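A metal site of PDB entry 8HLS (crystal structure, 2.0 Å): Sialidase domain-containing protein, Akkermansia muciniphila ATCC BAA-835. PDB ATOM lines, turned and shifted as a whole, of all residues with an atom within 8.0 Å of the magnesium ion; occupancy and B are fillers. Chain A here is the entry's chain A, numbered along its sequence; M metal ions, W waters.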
ATOM      1  N   HIS A 201      -5.443 -12.431   1.140  1.00  0.00           N
ATOM      2  CA  HIS A 201      -6.067 -13.546   1.836  1.00  0.00           C
ATOM      3  C   HIS A 201      -6.886 -13.022   3.018  1.00  0.00           C
ATOM      4  O   HIS A 201      -6.482 -12.076   3.700  1.00  0.00           O
ATOM      5  CB  HIS A 201      -4.992 -14.529   2.306  1.00  0.00           C
ATOM      6  CG  HIS A 201      -5.508 -15.626   3.200  1.00  0.00           C
ATOM      7  ND1 HIS A 201      -5.279 -15.638   4.561  1.00  0.00           N
ATOM      8  CD2 HIS A 201      -6.242 -16.725   2.927  1.00  0.00           C
ATOM      9  CE1 HIS A 201      -5.843 -16.711   5.091  1.00  0.00           C
ATOM     10  NE2 HIS A 201      -6.441 -17.387   4.120  1.00  0.00           N
ATOM     11  N   HIS A 207      -8.490 -20.706   9.196  1.00  0.00           N
ATOM     12  CA  HIS A 207      -7.381 -19.812   9.459  1.00  0.00           C
ATOM     13  C   HIS A 207      -7.619 -18.968  10.710  1.00  0.00           C
ATOM     14  O   HIS A 207      -8.732 -18.539  10.950  1.00  0.00           O
ATOM     15  CB  HIS A 207      -7.156 -18.895   8.263  1.00  0.00           C
ATOM     16  CG  HIS A 207      -6.767 -19.623   7.012  1.00  0.00           C
ATOM     17  ND1 HIS A 207      -5.511 -20.138   6.808  1.00  0.00           N
ATOM     18  CD2 HIS A 207      -7.484 -19.910   5.897  1.00  0.00           C
ATOM     19  CE1 HIS A 207      -5.463 -20.725   5.622  1.00  0.00           C
ATOM     20  NE2 HIS A 207      -6.645 -20.595   5.047  1.00  0.00           N
ATOM     21  N   GLY A 209      -5.425 -16.331  11.241  1.00  0.00           N
ATOM     22  CA  GLY A 209      -4.672 -15.154  10.881  1.00  0.00           C
ATOM     23  C   GLY A 209      -4.607 -15.104   9.375  1.00  0.00           C
ATOM     24  O   GLY A 209      -5.193 -15.938   8.687  1.00  0.00           O
ATOM     25  N   VAL A 210      -3.890 -14.103   8.866  1.00  0.00           N
ATOM     26  CA  VAL A 210      -3.837 -13.821   7.435  1.00  0.00           C
ATOM     27  C   VAL A 210      -2.515 -14.338   6.871  1.00  0.00           C
ATOM     28  O   VAL A 210      -1.453 -14.230   7.514  1.00  0.00           O
ATOM     29  CB  VAL A 210      -4.021 -12.305   7.174  1.00  0.00           C
ATOM     30  CG1 VAL A 210      -3.033 -11.523   7.973  1.00  0.00           C
ATOM     31  CG2 VAL A 210      -3.908 -11.965   5.704  1.00  0.00           C
ATOM     32  N   ARG A 211      -2.584 -14.928   5.684  1.00  0.00           N
ATOM     33  CA  ARG A 211      -1.372 -15.313   4.970  1.00  0.00           C
ATOM     34  C   ARG A 211      -0.564 -14.089   4.564  1.00  0.00           C
ATOM     35  O   ARG A 211      -1.110 -13.021   4.270  1.00  0.00           O
ATOM     36  CB  ARG A 211      -1.731 -16.094   3.700  1.00  0.00           C
ATOM     37  CG  ARG A 211      -2.036 -17.552   3.948  1.00  0.00           C
ATOM     38  CD  ARG A 211      -2.507 -18.216   2.657  1.00  0.00           C
ATOM     39  NE  ARG A 211      -3.076 -19.529   2.891  1.00  0.00           N
ATOM     40  CZ  ARG A 211      -3.971 -20.118   2.110  1.00  0.00           C
ATOM     41  NH1 ARG A 211      -4.442 -19.518   1.038  1.00  0.00           N
ATOM     42  NH2 ARG A 211      -4.409 -21.335   2.429  1.00  0.00           N
ATOM     43  N   TRP A 212       0.749 -14.264   4.499  1.00  0.00           N
ATOM     44  CA  TRP A 212       1.618 -13.239   3.933  1.00  0.00           C
ATOM     45  C   TRP A 212       1.115 -12.844   2.551  1.00  0.00           C
ATOM     46  O   TRP A 212       0.772 -13.700   1.729  1.00  0.00           O
ATOM     47  CB  TRP A 212       3.043 -13.803   3.858  1.00  0.00           C
ATOM     48  CG  TRP A 212       4.075 -12.903   3.263  1.00  0.00           C
ATOM     49  CD1 TRP A 212       4.150 -11.542   3.362  1.00  0.00           C
ATOM     50  CD2 TRP A 212       5.200 -13.309   2.463  1.00  0.00           C
ATOM     51  NE1 TRP A 212       5.254 -11.076   2.682  1.00  0.00           N
ATOM     52  CE2 TRP A 212       5.920 -12.144   2.117  1.00  0.00           C
ATOM     53  CE3 TRP A 212       5.666 -14.556   2.009  1.00  0.00           C
ATOM     54  CZ2 TRP A 212       7.084 -12.176   1.340  1.00  0.00           C
ATOM     55  CZ3 TRP A 212       6.831 -14.582   1.224  1.00  0.00           C
ATOM     56  CH2 TRP A 212       7.520 -13.412   0.904  1.00  0.00           C
ATOM     57  N   PHE A 213       0.976 -11.538   2.336  1.00  0.00           N
ATOM     58  CA  PHE A 213       0.393 -11.039   1.087  1.00  0.00           C
ATOM     59  C   PHE A 213       1.449 -10.980  -0.020  1.00  0.00           C
ATOM     60  O   PHE A 213       2.458 -10.275   0.104  1.00  0.00           O
ATOM     61  CB  PHE A 213      -0.247  -9.672   1.290  1.00  0.00           C
ATOM     62  CG  PHE A 213      -0.849  -9.098   0.035  1.00  0.00           C
ATOM     63  CD1 PHE A 213      -1.587  -9.901  -0.820  1.00  0.00           C
ATOM     64  CD2 PHE A 213      -0.646  -7.760  -0.302  1.00  0.00           C
ATOM     65  CE1 PHE A 213      -2.133  -9.388  -1.990  1.00  0.00           C
ATOM     66  CE2 PHE A 213      -1.196  -7.239  -1.466  1.00  0.00           C
ATOM     67  CZ  PHE A 213      -1.943  -8.051  -2.316  1.00  0.00           C
ATOM     68  N   LEU A 264       1.997 -19.274  -2.255  1.00  0.00           N
ATOM     69  CA  LEU A 264       3.286 -18.660  -1.974  1.00  0.00           C
ATOM     70  C   LEU A 264       4.435 -19.500  -2.523  1.00  0.00           C
ATOM     71  O   LEU A 264       5.510 -19.576  -1.930  1.00  0.00           O
ATOM     72  CB  LEU A 264       3.449 -18.395  -0.472  1.00  0.00           C
ATOM     73  CG  LEU A 264       2.364 -17.462   0.103  1.00  0.00           C
ATOM     74  CD1 LEU A 264       2.396 -17.359   1.647  1.00  0.00           C
ATOM     75  CD2 LEU A 264       2.469 -16.094  -0.547  1.00  0.00           C
ATOM     76  N   ALA A 286      -0.782 -25.328   2.297  1.00  0.00           N
ATOM     77  CA  ALA A 286      -0.114 -25.018   3.551  1.00  0.00           C
ATOM     78  C   ALA A 286      -1.060 -25.231   4.728  1.00  0.00           C
ATOM     79  O   ALA A 286      -2.288 -25.246   4.581  1.00  0.00           O
ATOM     80  CB  ALA A 286       0.390 -23.572   3.551  1.00  0.00           C
ATOM     81  N   LEU A 287      -0.486 -25.434   5.910  1.00  0.00           N
ATOM     82  CA  LEU A 287      -1.309 -25.498   7.111  1.00  0.00           C
ATOM     83  C   LEU A 287      -2.067 -24.183   7.288  1.00  0.00           C
ATOM     84  O   LEU A 287      -1.585 -23.112   6.887  1.00  0.00           O
ATOM     85  CB  LEU A 287      -0.450 -25.768   8.344  1.00  0.00           C
ATOM     86  CG  LEU A 287       0.035 -27.207   8.577  1.00  0.00           C
ATOM     87  CD1 LEU A 287       1.006 -27.233   9.715  1.00  0.00           C
ATOM     88  CD2 LEU A 287      -1.099 -28.168   8.852  1.00  0.00           C
ATOM     89  N   PRO A 288      -3.254 -24.220   7.884  1.00  0.00           N
ATOM     90  CA  PRO A 288      -3.983 -22.967   8.130  1.00  0.00           C
ATOM     91  C   PRO A 288      -3.126 -22.017   8.956  1.00  0.00           C
ATOM     92  O   PRO A 288      -2.312 -22.455   9.780  1.00  0.00           O
ATOM     93  CB  PRO A 288      -5.221 -23.421   8.921  1.00  0.00           C
ATOM     94  CG  PRO A 288      -5.350 -24.870   8.688  1.00  0.00           C
ATOM     95  CD  PRO A 288      -3.955 -25.389   8.456  1.00  0.00           C
ATOM     96  N   GLU A 289      -3.270 -20.721   8.696  1.00  0.00           N
ATOM     97  CA  GLU A 289      -2.567 -19.705   9.470  1.00  0.00           C
ATOM     98  C   GLU A 289      -2.934 -19.805  10.948  1.00  0.00           C
ATOM     99  O   GLU A 289      -4.087 -20.092  11.306  1.00  0.00           O
ATOM    100  CB  GLU A 289      -2.909 -18.309   8.952  1.00  0.00           C
ATOM    101  CG  GLU A 289      -2.367 -18.067   7.547  1.00  0.00           C
ATOM    102  CD  GLU A 289      -0.879 -18.463   7.430  1.00  0.00           C
ATOM    103  OE1 GLU A 289      -0.033 -17.809   8.105  1.00  0.00           O
ATOM    104  OE2 GLU A 289      -0.550 -19.423   6.665  1.00  0.00           O
ATOM    105  N   ASN A 290      -1.946 -19.612  11.827  1.00  0.00           N
ATOM    106  CA  ASN A 290      -2.191 -19.764  13.240  1.00  0.00           C
ATOM    107  C   ASN A 290      -2.507 -18.398  13.874  1.00  0.00           C
ATOM    108  O   ASN A 290      -2.613 -17.381  13.177  1.00  0.00           O
ATOM    109  CB  ASN A 290      -1.010 -20.488  13.903  1.00  0.00           C
ATOM    110  CG  ASN A 290       0.298 -19.696  13.855  1.00  0.00           C
ATOM    111  OD1 ASN A 290       0.310 -18.465  13.924  1.00  0.00           O
ATOM    112  ND2 ASN A 290       1.404 -20.422  13.767  1.00  0.00           N
ATOM    113  N   THR A 292      -0.880 -16.343  15.636  1.00  0.00           N
ATOM    114  CA  THR A 292       0.142 -15.307  15.660  1.00  0.00           C
ATOM    115  C   THR A 292       0.723 -15.036  14.280  1.00  0.00           C
ATOM    116  O   THR A 292       1.879 -14.661  14.153  1.00  0.00           O
ATOM    117  CB  THR A 292       1.285 -15.681  16.624  1.00  0.00           C
ATOM    118  OG1 THR A 292       1.859 -16.927  16.206  1.00  0.00           O
ATOM    119  CG2 THR A 292       0.792 -15.794  18.069  1.00  0.00           C
ATOM    120  N   ALA A 293      -0.096 -15.181  13.227  1.00  0.00           N
ATOM    121  CA  ALA A 293       0.385 -15.132  11.845  1.00  0.00           C
ATOM    122  C   ALA A 293       0.868 -13.752  11.440  1.00  0.00           C
ATOM    123  O   ALA A 293       1.730 -13.628  10.553  1.00  0.00           O
ATOM    124  CB  ALA A 293      -0.732 -15.572  10.905  1.00  0.00           C
ATOM    125  N   GLY A 294       0.307 -12.705  12.035  1.00  0.00           N
ATOM    126  CA  GLY A 294       0.643 -11.350  11.674  1.00  0.00           C
ATOM    127  C   GLY A 294      -0.440 -10.686  10.847  1.00  0.00           C
ATOM    128  O   GLY A 294      -1.565 -11.179  10.698  1.00  0.00           O
ATOM    129  N   GLY A 296      -0.091  -9.936   7.581  1.00  0.00           N
ATOM    130  CA  GLY A 296       0.067 -10.221   6.181  1.00  0.00           C
ATOM    131  C   GLY A 296       1.196  -9.474   5.516  1.00  0.00           C
ATOM    132  O   GLY A 296       1.420  -9.675   4.323  1.00  0.00           O
ATOM    133  N   TRP A 298       4.364  -9.829   6.564  1.00  0.00           N
ATOM    134  CA  TRP A 298       5.556 -10.671   6.659  1.00  0.00           C
ATOM    135  C   TRP A 298       5.117 -12.126   6.847  1.00  0.00           C
ATOM    136  O   TRP A 298       3.986 -12.404   7.265  1.00  0.00           O
ATOM    137  CB  TRP A 298       6.475 -10.214   7.808  1.00  0.00           C
ATOM    138  CG  TRP A 298       5.716 -10.006   9.083  1.00  0.00           C
ATOM    139  CD1 TRP A 298       5.002  -8.897   9.448  1.00  0.00           C
ATOM    140  CD2 TRP A 298       5.589 -10.940  10.150  1.00  0.00           C
ATOM    141  NE1 TRP A 298       4.427  -9.081  10.693  1.00  0.00           N
ATOM    142  CE2 TRP A 298       4.771 -10.334  11.143  1.00  0.00           C
ATOM    143  CE3 TRP A 298       6.076 -12.225  10.374  1.00  0.00           C
ATOM    144  CZ2 TRP A 298       4.450 -10.972  12.329  1.00  0.00           C
ATOM    145  CZ3 TRP A 298       5.745 -12.867  11.557  1.00  0.00           C
ATOM    146  CH2 TRP A 298       4.939 -12.240  12.530  1.00  0.00           C
ATOM    147  N   GLU A 299       6.012 -13.051   6.501  1.00  0.00           N
ATOM    148  CA  GLU A 299       5.717 -14.467   6.605  1.00  0.00           C
ATOM    149  C   GLU A 299       6.201 -15.009   7.937  1.00  0.00           C
ATOM    150  O   GLU A 299       7.304 -14.704   8.370  1.00  0.00           O
ATOM    151  CB  GLU A 299       6.391 -15.257   5.472  1.00  0.00           C
ATOM    152  CG  GLU A 299       6.080 -16.752   5.490  1.00  0.00           C
ATOM    153  CD  GLU A 299       4.585 -17.053   5.630  1.00  0.00           C
ATOM    154  OE1 GLU A 299       4.066 -17.053   6.768  1.00  0.00           O
ATOM    155  OE2 GLU A 299       3.925 -17.308   4.583  1.00  0.00           O
ATOM    156  N   ASP A 300       5.371 -15.827   8.576  1.00  0.00           N
ATOM    157  CA  ASP A 300       5.772 -16.429   9.842  1.00  0.00           C
ATOM    158  C   ASP A 300       6.386 -17.818   9.671  1.00  0.00           C
ATOM    159  O   ASP A 300       7.377 -18.135  10.337  1.00  0.00           O
ATOM    160  CB  ASP A 300       4.589 -16.462  10.844  1.00  0.00           C
ATOM    161  CG  ASP A 300       3.350 -17.252  10.345  1.00  0.00           C
ATOM    162  OD1 ASP A 300       2.903 -17.074   9.193  1.00  0.00           O
ATOM    163  OD2 ASP A 300       2.793 -18.029  11.153  1.00  0.00           O
ATOM    164  N   VAL A 301       5.853 -18.650   8.775  1.00  0.00           N
ATOM    165  CA  VAL A 301       6.410 -19.992   8.571  1.00  0.00           C
ATOM    166  C   VAL A 301       5.929 -20.534   7.234  1.00  0.00           C
ATOM    167  O   VAL A 301       4.796 -20.271   6.802  1.00  0.00           O
ATOM    168  CB  VAL A 301       6.042 -20.947   9.740  1.00  0.00           C
ATOM    169  CG1 VAL A 301       4.535 -21.155   9.836  1.00  0.00           C
ATOM    170  CG2 VAL A 301       6.756 -22.282   9.581  1.00  0.00           C
ATOM    171  N   PHE A 302       6.802 -21.309   6.570  1.00  0.00           N
ATOM    172  CA  PHE A 302       6.471 -22.046   5.349  1.00  0.00           C
ATOM    173  C   PHE A 302       6.276 -23.517   5.711  1.00  0.00           C
ATOM    174  O   PHE A 302       7.174 -24.155   6.263  1.00  0.00           O
ATOM    175  CB  PHE A 302       7.586 -21.924   4.307  1.00  0.00           C
ATOM    176  CG  PHE A 302       7.828 -20.531   3.827  1.00  0.00           C
ATOM    177  CD1 PHE A 302       6.883 -19.877   3.056  1.00  0.00           C
ATOM    178  CD2 PHE A 302       9.018 -19.879   4.116  1.00  0.00           C
ATOM    179  CE1 PHE A 302       7.109 -18.595   2.591  1.00  0.00           C
ATOM    180  CE2 PHE A 302       9.253 -18.595   3.653  1.00  0.00           C
ATOM    181  CZ  PHE A 302       8.289 -17.952   2.884  1.00  0.00           C
ATOM    182  N   THR A 303       5.093 -24.059   5.368  1.00  0.00           N
ATOM    183  CA  THR A 303       4.746 -25.440   5.646  1.00  0.00           C
ATOM    184  C   THR A 303       4.323 -26.196   4.389  1.00  0.00           C
ATOM    185  O   THR A 303       3.588 -27.184   4.478  1.00  0.00           O
ATOM    186  CB  THR A 303       3.626 -25.523   6.705  1.00  0.00           C
ATOM    187  OG1 THR A 303       2.437 -24.903   6.200  1.00  0.00           O
ATOM    188  CG2 THR A 303       4.029 -24.821   8.006  1.00  0.00           C
ATOM    189  N   TYR A 414       9.822 -24.604  10.432  1.00  0.00           N
ATOM    190  CA  TYR A 414       9.567 -25.423  11.600  1.00  0.00           C
ATOM    191  C   TYR A 414      10.463 -26.655  11.498  1.00  0.00           C
ATOM    192  O   TYR A 414      10.639 -27.212  10.397  1.00  0.00           O
ATOM    193  CB  TYR A 414       8.118 -25.889  11.669  1.00  0.00           C
ATOM    194  CG  TYR A 414       7.050 -24.892  12.093  1.00  0.00           C
ATOM    195  CD1 TYR A 414       7.338 -23.798  12.914  1.00  0.00           C
ATOM    196  CD2 TYR A 414       5.728 -25.102  11.726  1.00  0.00           C
ATOM    197  CE1 TYR A 414       6.309 -22.909  13.310  1.00  0.00           C
ATOM    198  CE2 TYR A 414       4.730 -24.250  12.121  1.00  0.00           C
ATOM    199  CZ  TYR A 414       5.015 -23.148  12.911  1.00  0.00           C
ATOM    200  OH  TYR A 414       3.968 -22.338  13.257  1.00  0.00           O
HETATM  201 MG    MG M   1       1.879 -17.259   7.499  1.00  0.00          MG
HETATM  202  O   HOH W   1       1.443 -15.207   7.611  1.00  0.00           O
HETATM  203  O   HOH W   2       2.273 -19.455   7.411  1.00  0.00           O
HETATM  204  O   HOH W   3       1.412 -17.456   5.265  1.00  0.00           O
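Water W1 lies within hydrogen-bond range of the backbone carbonyl oxygen (O) of Val 210, the backbone NH (N) of Trp 212 and the backbone carbonyl oxygen (O) of Ala 293.
Water W2 lies within hydrogen-bond range of O of Val 301 and OE2 of Glu 289.
Water W3 lies within hydrogen-bond range of OE2 of Glu 299 (2.6 Å), OE2 of Glu 289 (3.1 Å) and N of Trp 212 (3.3 Å).
N of Val 301 lies close to OE1 of Glu 299.
The backbone NH (N) of Glu 289 sits at hydrogen-bond distance from a ring nitrogen (ND1) of His 207, 3.0 Å away.
The magnesium ion is bound by the side-chain carboxylate (OD1) of Asp 300 (2.0 Å), the side-chain carboxylate (OE1) of Glu 289 (2.1 Å), water W1 (2.1 Å), water W2 (2.2 Å), water W3 (2.3 Å) and the side-chain carboxylate (OE1) of Glu 299 (2.3 Å).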
